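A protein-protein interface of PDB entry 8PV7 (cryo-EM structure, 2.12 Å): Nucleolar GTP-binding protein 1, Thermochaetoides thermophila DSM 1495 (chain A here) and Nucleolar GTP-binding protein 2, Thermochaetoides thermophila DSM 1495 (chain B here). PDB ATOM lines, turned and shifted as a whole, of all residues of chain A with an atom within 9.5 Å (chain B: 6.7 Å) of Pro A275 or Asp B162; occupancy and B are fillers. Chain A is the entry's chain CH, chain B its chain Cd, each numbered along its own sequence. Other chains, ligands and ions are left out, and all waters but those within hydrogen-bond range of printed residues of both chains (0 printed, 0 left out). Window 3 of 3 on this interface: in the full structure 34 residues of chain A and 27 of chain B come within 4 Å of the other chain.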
ATOM      1  N   LEU A 228       0.663  22.905 -11.915  1.00  0.00           N
ATOM      2  CA  LEU A 228       1.905  23.507 -12.390  1.00  0.00           C
ATOM      3  C   LEU A 228       2.548  22.699 -13.508  1.00  0.00           C
ATOM      4  O   LEU A 228       3.246  23.259 -14.360  1.00  0.00           O
ATOM      5  CB  LEU A 228       2.890  23.666 -11.234  1.00  0.00           C
ATOM      6  CG  LEU A 228       2.541  24.652 -10.123  1.00  0.00           C
ATOM      7  CD1 LEU A 228       3.539  24.507  -9.002  1.00  0.00           C
ATOM      8  CD2 LEU A 228       2.531  26.076 -10.636  1.00  0.00           C
ATOM      9  N   LEU A 242       4.856  35.631  -8.956  1.00  0.00           N
ATOM     10  CA  LEU A 242       4.053  35.474  -7.745  1.00  0.00           C
ATOM     11  C   LEU A 242       4.796  34.714  -6.657  1.00  0.00           C
ATOM     12  O   LEU A 242       4.593  34.986  -5.472  1.00  0.00           O
ATOM     13  CB  LEU A 242       2.747  34.754  -8.058  1.00  0.00           C
ATOM     14  CG  LEU A 242       1.662  35.501  -8.820  1.00  0.00           C
ATOM     15  CD1 LEU A 242       0.659  34.512  -9.361  1.00  0.00           C
ATOM     16  CD2 LEU A 242       0.986  36.506  -7.919  1.00  0.00           C
ATOM     17  N   ALA A 243       5.633  33.754  -7.028  1.00  0.00           N
ATOM     18  CA  ALA A 243       6.332  32.957  -6.033  1.00  0.00           C
ATOM     19  C   ALA A 243       7.545  33.656  -5.443  1.00  0.00           C
ATOM     20  O   ALA A 243       7.845  33.451  -4.262  1.00  0.00           O
ATOM     21  CB  ALA A 243       6.762  31.619  -6.632  1.00  0.00           C
ATOM     22  N   ASN A 268     -11.441  29.381  -7.870  1.00  0.00           N
ATOM     23  CA  ASN A 268     -10.629  28.183  -7.675  1.00  0.00           C
ATOM     24  C   ASN A 268      -9.160  28.440  -7.983  1.00  0.00           C
ATOM     25  O   ASN A 268      -8.280  27.887  -7.316  1.00  0.00           O
ATOM     26  CB  ASN A 268     -11.162  27.037  -8.530  1.00  0.00           C
ATOM     27  CG  ASN A 268     -12.524  26.562  -8.082  1.00  0.00           C
ATOM     28  OD1 ASN A 268     -12.971  26.878  -6.979  1.00  0.00           O
ATOM     29  ND2 ASN A 268     -13.198  25.805  -8.937  1.00  0.00           N
ATOM     30  N   LEU A 269      -8.873  29.281  -8.978  1.00  0.00           N
ATOM     31  CA  LEU A 269      -7.489  29.657  -9.249  1.00  0.00           C
ATOM     32  C   LEU A 269      -6.896  30.436  -8.081  1.00  0.00           C
ATOM     33  O   LEU A 269      -5.734  30.223  -7.700  1.00  0.00           O
ATOM     34  CB  LEU A 269      -7.401  30.478 -10.535  1.00  0.00           C
ATOM     35  CG  LEU A 269      -5.977  30.945 -10.847  1.00  0.00           C
ATOM     36  CD1 LEU A 269      -5.065  29.744 -11.019  1.00  0.00           C
ATOM     37  CD2 LEU A 269      -5.910  31.854 -12.055  1.00  0.00           C
ATOM     38  N   PHE A 270      -7.685  31.345  -7.499  1.00  0.00           N
ATOM     39  CA  PHE A 270      -7.214  32.093  -6.337  1.00  0.00           C
ATOM     40  C   PHE A 270      -6.902  31.167  -5.164  1.00  0.00           C
ATOM     41  O   PHE A 270      -5.852  31.295  -4.521  1.00  0.00           O
ATOM     42  CB  PHE A 270      -8.245  33.146  -5.929  1.00  0.00           C
ATOM     43  CG  PHE A 270      -7.832  33.950  -4.735  1.00  0.00           C
ATOM     44  CD1 PHE A 270      -6.910  34.972  -4.864  1.00  0.00           C
ATOM     45  CD2 PHE A 270      -8.346  33.671  -3.480  1.00  0.00           C
ATOM     46  CE1 PHE A 270      -6.518  35.702  -3.768  1.00  0.00           C
ATOM     47  CE2 PHE A 270      -7.951  34.400  -2.381  1.00  0.00           C
ATOM     48  CZ  PHE A 270      -7.038  35.417  -2.525  1.00  0.00           C
ATOM     49  N   LYS A 271      -7.798  30.219  -4.877  1.00  0.00           N
ATOM     50  CA  LYS A 271      -7.549  29.280  -3.782  1.00  0.00           C
ATOM     51  C   LYS A 271      -6.372  28.361  -4.088  1.00  0.00           C
ATOM     52  O   LYS A 271      -5.654  27.940  -3.177  1.00  0.00           O
ATOM     53  CB  LYS A 271      -8.802  28.458  -3.477  1.00  0.00           C
ATOM     54  CG  LYS A 271     -10.065  29.270  -3.317  1.00  0.00           C
ATOM     55  CD  LYS A 271     -10.828  28.898  -2.071  1.00  0.00           C
ATOM     56  CE  LYS A 271     -11.459  27.529  -2.218  1.00  0.00           C
ATOM     57  NZ  LYS A 271     -12.798  27.605  -2.861  1.00  0.00           N
ATOM     58  N   SER A 272      -6.160  28.040  -5.365  1.00  0.00           N
ATOM     59  CA  SER A 272      -5.028  27.203  -5.742  1.00  0.00           C
ATOM     60  C   SER A 272      -3.699  27.914  -5.511  1.00  0.00           C
ATOM     61  O   SER A 272      -2.743  27.306  -5.018  1.00  0.00           O
ATOM     62  CB  SER A 272      -5.158  26.782  -7.202  1.00  0.00           C
ATOM     63  OG  SER A 272      -3.982  26.134  -7.644  1.00  0.00           O
ATOM     64  N   ILE A 273      -3.611  29.203  -5.860  1.00  0.00           N
ATOM     65  CA  ILE A 273      -2.339  29.909  -5.717  1.00  0.00           C
ATOM     66  C   ILE A 273      -2.207  30.632  -4.386  1.00  0.00           C
ATOM     67  O   ILE A 273      -1.202  31.322  -4.171  1.00  0.00           O
ATOM     68  CB  ILE A 273      -2.100  30.925  -6.851  1.00  0.00           C
ATOM     69  CG1 ILE A 273      -3.135  32.047  -6.795  1.00  0.00           C
ATOM     70  CG2 ILE A 273      -2.098  30.222  -8.198  1.00  0.00           C
ATOM     71  CD1 ILE A 273      -3.082  32.987  -7.971  1.00  0.00           C
ATOM     72  N   LYS A 274      -3.194  30.509  -3.497  1.00  0.00           N
ATOM     73  CA  LYS A 274      -3.104  31.133  -2.177  1.00  0.00           C
ATOM     74  C   LYS A 274      -1.886  30.742  -1.330  1.00  0.00           C
ATOM     75  O   LYS A 274      -1.389  31.623  -0.608  1.00  0.00           O
ATOM     76  CB  LYS A 274      -4.407  30.874  -1.409  1.00  0.00           C
ATOM     77  CG  LYS A 274      -4.670  31.859  -0.294  1.00  0.00           C
ATOM     78  CD  LYS A 274      -6.134  31.878   0.087  1.00  0.00           C
ATOM     79  CE  LYS A 274      -6.424  32.971   1.099  1.00  0.00           C
ATOM     80  NZ  LYS A 274      -7.886  33.110   1.351  1.00  0.00           N
ATOM     81  N   PRO A 275      -1.377  29.493  -1.322  1.00  0.00           N
ATOM     82  CA  PRO A 275      -0.139  29.233  -0.557  1.00  0.00           C
ATOM     83  C   PRO A 275       1.079  30.036  -0.999  1.00  0.00           C
ATOM     84  O   PRO A 275       2.010  30.203  -0.202  1.00  0.00           O
ATOM     85  CB  PRO A 275       0.097  27.728  -0.752  1.00  0.00           C
ATOM     86  CG  PRO A 275      -0.986  27.238  -1.622  1.00  0.00           C
ATOM     87  CD  PRO A 275      -2.076  28.225  -1.595  1.00  0.00           C
ATOM     88  N   LEU A 276       1.110  30.539  -2.234  1.00  0.00           N
ATOM     89  CA  LEU A 276       2.167  31.457  -2.641  1.00  0.00           C
ATOM     90  C   LEU A 276       2.045  32.822  -1.980  1.00  0.00           C
ATOM     91  O   LEU A 276       3.010  33.590  -1.994  1.00  0.00           O
ATOM     92  CB  LEU A 276       2.163  31.651  -4.157  1.00  0.00           C
ATOM     93  CG  LEU A 276       2.545  30.465  -5.038  1.00  0.00           C
ATOM     94  CD1 LEU A 276       2.612  30.887  -6.489  1.00  0.00           C
ATOM     95  CD2 LEU A 276       3.847  29.829  -4.584  1.00  0.00           C
ATOM     96  N   PHE A 277       0.884  33.141  -1.413  1.00  0.00           N
ATOM     97  CA  PHE A 277       0.612  34.473  -0.896  1.00  0.00           C
ATOM     98  C   PHE A 277       0.985  34.632   0.567  1.00  0.00           C
ATOM     99  O   PHE A 277       0.576  35.624   1.181  1.00  0.00           O
ATOM    100  CB  PHE A 277      -0.866  34.815  -1.073  1.00  0.00           C
ATOM    101  CG  PHE A 277      -1.294  34.947  -2.502  1.00  0.00           C
ATOM    102  CD1 PHE A 277      -0.384  35.272  -3.490  1.00  0.00           C
ATOM    103  CD2 PHE A 277      -2.614  34.743  -2.856  1.00  0.00           C
ATOM    104  CE1 PHE A 277      -0.783  35.384  -4.799  1.00  0.00           C
ATOM    105  CE2 PHE A 277      -3.016  34.861  -4.162  1.00  0.00           C
ATOM    106  CZ  PHE A 277      -2.100  35.181  -5.134  1.00  0.00           C
ATOM    107  N   ALA A 278       1.712  33.679   1.143  1.00  0.00           N
ATOM    108  CA  ALA A 278       2.222  33.848   2.494  1.00  0.00           C
ATOM    109  C   ALA A 278       3.195  35.019   2.537  1.00  0.00           C
ATOM    110  O   ALA A 278       3.882  35.313   1.555  1.00  0.00           O
ATOM    111  CB  ALA A 278       2.907  32.571   2.974  1.00  0.00           C
ATOM    112  N   ASN A 279       3.205  35.711   3.679  1.00  0.00           N
ATOM    113  CA  ASN A 279       3.910  36.965   3.965  1.00  0.00           C
ATOM    114  C   ASN A 279       3.755  38.021   2.873  1.00  0.00           C
ATOM    115  O   ASN A 279       4.660  38.843   2.679  1.00  0.00           O
ATOM    116  CB  ASN A 279       5.398  36.739   4.300  1.00  0.00           C
ATOM    117  CG  ASN A 279       6.237  36.298   3.110  1.00  0.00           C
ATOM    118  OD1 ASN A 279       6.373  35.104   2.840  1.00  0.00           O
ATOM    119  ND2 ASN A 279       6.810  37.262   2.398  1.00  0.00           N
ATOM    120  N   LYS A 280       2.624  38.042   2.167  1.00  0.00           N
ATOM    121  CA  LYS A 280       2.311  39.084   1.200  1.00  0.00           C
ATOM    122  C   LYS A 280       0.885  39.556   1.440  1.00  0.00           C
ATOM    123  O   LYS A 280       0.043  38.813   1.949  1.00  0.00           O
ATOM    124  CB  LYS A 280       2.468  38.599  -0.254  1.00  0.00           C
ATOM    125  CG  LYS A 280       3.792  37.911  -0.549  1.00  0.00           C
ATOM    126  CD  LYS A 280       3.878  37.366  -1.961  1.00  0.00           C
ATOM    127  CE  LYS A 280       5.112  36.483  -2.096  1.00  0.00           C
ATOM    128  NZ  LYS A 280       5.343  35.987  -3.473  1.00  0.00           N
ATOM    129  N   VAL A 282      -2.725  40.686  -0.009  1.00  0.00           N
ATOM    130  CA  VAL A 282      -3.533  40.234  -1.134  1.00  0.00           C
ATOM    131  C   VAL A 282      -4.791  41.083  -1.238  1.00  0.00           C
ATOM    132  O   VAL A 282      -5.546  41.237  -0.267  1.00  0.00           O
ATOM    133  CB  VAL A 282      -3.904  38.744  -1.010  1.00  0.00           C
ATOM    134  CG1 VAL A 282      -4.487  38.244  -2.310  1.00  0.00           C
ATOM    135  CG2 VAL A 282      -2.696  37.925  -0.630  1.00  0.00           C
ATOM    136  N   GLU A 313      -6.755  38.285   5.747  1.00  0.00           N
ATOM    137  CA  GLU A 313      -5.538  38.603   5.012  1.00  0.00           C
ATOM    138  C   GLU A 313      -5.799  39.072   3.586  1.00  0.00           C
ATOM    139  O   GLU A 313      -4.851  39.462   2.897  1.00  0.00           O
ATOM    140  CB  GLU A 313      -4.614  37.385   4.991  1.00  0.00           C
ATOM    141  CG  GLU A 313      -5.333  36.084   4.690  1.00  0.00           C
ATOM    142  CD  GLU A 313      -4.491  34.866   5.005  1.00  0.00           C
ATOM    143  OE1 GLU A 313      -3.321  35.039   5.404  1.00  0.00           O
ATOM    144  OE2 GLU A 313      -5.000  33.735   4.856  1.00  0.00           O
ATOM    145  N   ASN B 159       6.583  20.282  -8.002  1.00  0.00           N
ATOM    146  CA  ASN B 159       5.384  19.768  -8.639  1.00  0.00           C
ATOM    147  C   ASN B 159       4.094  20.360  -8.096  1.00  0.00           C
ATOM    148  O   ASN B 159       3.082  20.331  -8.802  1.00  0.00           O
ATOM    149  CB  ASN B 159       5.320  18.239  -8.507  1.00  0.00           C
ATOM    150  CG  ASN B 159       6.123  17.539  -9.571  1.00  0.00           C
ATOM    151  OD1 ASN B 159       7.289  17.206  -9.365  1.00  0.00           O
ATOM    152  ND2 ASN B 159       5.509  17.320 -10.726  1.00  0.00           N
ATOM    153  N   THR B 160       4.093  20.876  -6.872  1.00  0.00           N
ATOM    154  CA  THR B 160       2.914  21.486  -6.284  1.00  0.00           C
ATOM    155  C   THR B 160       3.217  22.927  -5.900  1.00  0.00           C
ATOM    156  O   THR B 160       4.375  23.347  -5.818  1.00  0.00           O
ATOM    157  CB  THR B 160       2.419  20.719  -5.044  1.00  0.00           C
ATOM    158  OG1 THR B 160       3.249  21.034  -3.921  1.00  0.00           O
ATOM    159  CG2 THR B 160       2.438  19.219  -5.280  1.00  0.00           C
ATOM    160  N   VAL B 161       2.141  23.678  -5.662  1.00  0.00           N
ATOM    161  CA  VAL B 161       2.256  25.069  -5.235  1.00  0.00           C
ATOM    162  C   VAL B 161       2.882  25.154  -3.845  1.00  0.00           C
ATOM    163  O   VAL B 161       3.652  26.077  -3.547  1.00  0.00           O
ATOM    164  CB  VAL B 161       0.871  25.741  -5.302  1.00  0.00           C
ATOM    165  CG1 VAL B 161       0.917  27.168  -4.810  1.00  0.00           C
ATOM    166  CG2 VAL B 161       0.348  25.702  -6.722  1.00  0.00           C
ATOM    167  N   ASP B 162       2.572  24.188  -2.975  1.00  0.00           N
ATOM    168  CA  ASP B 162       3.184  24.154  -1.648  1.00  0.00           C
ATOM    169  C   ASP B 162       4.686  23.908  -1.731  1.00  0.00           C
ATOM    170  O   ASP B 162       5.476  24.552  -1.022  1.00  0.00           O
ATOM    171  CB  ASP B 162       2.517  23.076  -0.798  1.00  0.00           C
ATOM    172  CG  ASP B 162       1.119  23.455  -0.374  1.00  0.00           C
ATOM    173  OD1 ASP B 162       0.974  24.118   0.674  1.00  0.00           O
ATOM    174  OD2 ASP B 162       0.162  23.094  -1.088  1.00  0.00           O
ATOM    175  N   GLU B 163       5.096  22.980  -2.599  1.00  0.00           N
ATOM    176  CA  GLU B 163       6.517  22.765  -2.843  1.00  0.00           C
ATOM    177  C   GLU B 163       7.169  24.002  -3.429  1.00  0.00           C
ATOM    178  O   GLU B 163       8.323  24.295  -3.114  1.00  0.00           O
ATOM    179  CB  GLU B 163       6.727  21.578  -3.777  1.00  0.00           C
ATOM    180  CG  GLU B 163       6.401  20.236  -3.169  1.00  0.00           C
ATOM    181  CD  GLU B 163       6.406  19.131  -4.199  1.00  0.00           C
ATOM    182  OE1 GLU B 163       6.502  19.445  -5.403  1.00  0.00           O
ATOM    183  OE2 GLU B 163       6.321  17.948  -3.809  1.00  0.00           O
ATOM    184  N   LEU B 164       6.452  24.734  -4.283  1.00  0.00           N
ATOM    185  CA  LEU B 164       6.992  25.968  -4.840  1.00  0.00           C
ATOM    186  C   LEU B 164       7.212  27.020  -3.759  1.00  0.00           C
ATOM    187  O   LEU B 164       8.220  27.732  -3.778  1.00  0.00           O
ATOM    188  CB  LEU B 164       6.060  26.494  -5.927  1.00  0.00           C
ATOM    189  CG  LEU B 164       6.342  27.862  -6.543  1.00  0.00           C
ATOM    190  CD1 LEU B 164       7.759  27.969  -7.067  1.00  0.00           C
ATOM    191  CD2 LEU B 164       5.349  28.126  -7.646  1.00  0.00           C
ATOM    192  N   ALA B 165       6.277  27.135  -2.816  1.00  0.00           N
ATOM    193  CA  ALA B 165       6.444  28.085  -1.718  1.00  0.00           C
ATOM    194  C   ALA B 165       7.644  27.721  -0.845  1.00  0.00           C
ATOM    195  O   ALA B 165       8.467  28.589  -0.507  1.00  0.00           O
ATOM    196  CB  ALA B 165       5.166  28.148  -0.886  1.00  0.00           C
ATOM    197  N   GLY B 166       7.779  26.435  -0.506  1.00  0.00           N
ATOM    198  CA  GLY B 166       8.944  26.001   0.253  1.00  0.00           C
ATOM    199  C   GLY B 166      10.244  26.195  -0.506  1.00  0.00           C
ATOM    200  O   GLY B 166      11.266  26.582   0.074  1.00  0.00           O
ATOM    201  N   TYR B 167      10.213  25.945  -1.815  1.00  0.00           N
ATOM    202  CA  TYR B 167      11.388  26.107  -2.659  1.00  0.00           C
ATOM    203  C   TYR B 167      11.818  27.561  -2.732  1.00  0.00           C
ATOM    204  O   TYR B 167      13.015  27.860  -2.696  1.00  0.00           O
ATOM    205  CB  TYR B 167      11.086  25.557  -4.052  1.00  0.00           C
ATOM    206  CG  TYR B 167      12.084  25.933  -5.113  1.00  0.00           C
ATOM    207  CD1 TYR B 167      13.321  25.312  -5.175  1.00  0.00           C
ATOM    208  CD2 TYR B 167      11.786  26.900  -6.065  1.00  0.00           C
ATOM    209  CE1 TYR B 167      14.236  25.645  -6.147  1.00  0.00           C
ATOM    210  CE2 TYR B 167      12.694  27.243  -7.035  1.00  0.00           C
ATOM    211  CZ  TYR B 167      13.918  26.611  -7.074  1.00  0.00           C
ATOM    212  OH  TYR B 167      14.833  26.943  -8.044  1.00  0.00           O
ATOM    213  N   GLU B 169      11.218  29.864  -0.434  1.00  0.00           N
ATOM    214  CA  GLU B 169      11.764  30.205   0.881  1.00  0.00           C
ATOM    215  C   GLU B 169      13.210  29.738   1.028  1.00  0.00           C
ATOM    216  O   GLU B 169      14.092  30.512   1.429  1.00  0.00           O
ATOM    217  CB  GLU B 169      10.897  29.592   1.976  1.00  0.00           C
ATOM    218  CG  GLU B 169      10.046  30.590   2.717  1.00  0.00           C
ATOM    219  CD  GLU B 169       8.742  29.991   3.195  1.00  0.00           C
ATOM    220  OE1 GLU B 169       7.901  30.744   3.728  1.00  0.00           O
ATOM    221  OE2 GLU B 169       8.558  28.767   3.038  1.00  0.00           O
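The backbone NH of Glu B163 is in hydrogen-bond range of the side-chain hydroxyl of Thr B160, at 3.0 Å.
The side-chain hydroxyl (OG1) of Thr B160 lies close to the backbone NH (N) of Asp B162, at 3.4 Å.
Leu A228 touches Thr B160.
CD1 of Leu A228 touches N of Val B161 (3.7 Å).
CB of Ala A243 touches CG of Leu B164, 3.8 Å away.
O of Ser A272 touches CG1 of Val B161, 3.7 Å away.
CG of Pro A275 touches CG1 of Val B161 (3.7 Å).
Asp B162 touches Pro A275 (OD1 to CB, 3.98 Å).
CB of Ala B165 touches O of Pro A275 (3.8 Å).
Leu A276 touches Val B161 (CG to CG1, 3.7 Å).
CD2 of Leu A276 touches CG of Leu B164, at 3.7 Å.
Printed residues of chain B within 4 Å of Leu A228: Thr B160 and Val B161.
Leu A242 touches none of the printed residues of chain B.
Of the printed residues of chain B, Ala A243 touches Leu B164 (3.8 Å).
Of the printed residues of chain B, Ser A272 touches Val B161 (3.7 Å).
Of chain A, only Leu A228, Ser A272, Pro A275 and Leu A276 come within 4 Å of Val B161.
Of chain A, only Pro A275 comes within 4 Å of Asp B162.
Glu B169 touches none of the printed residues of chain A.
The nearest printed residue of chain B that does not touch Pro A275 is Gly B166 (6.9 Å).
The nearest residue of chain A that does not touch Asp B162 is Leu A276 (6.0 Å).
Hydrophobic or aromatic side chains of chain A that line the printed part of chain B: Leu A228, Ala A243, Pro A275 and Leu A276.
Along chain A the printed residues that touch a printed residue of chain B span positions 228 to 276.
Of the 10 printed residues of chain B, 5 touch a printed residue of chain A.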
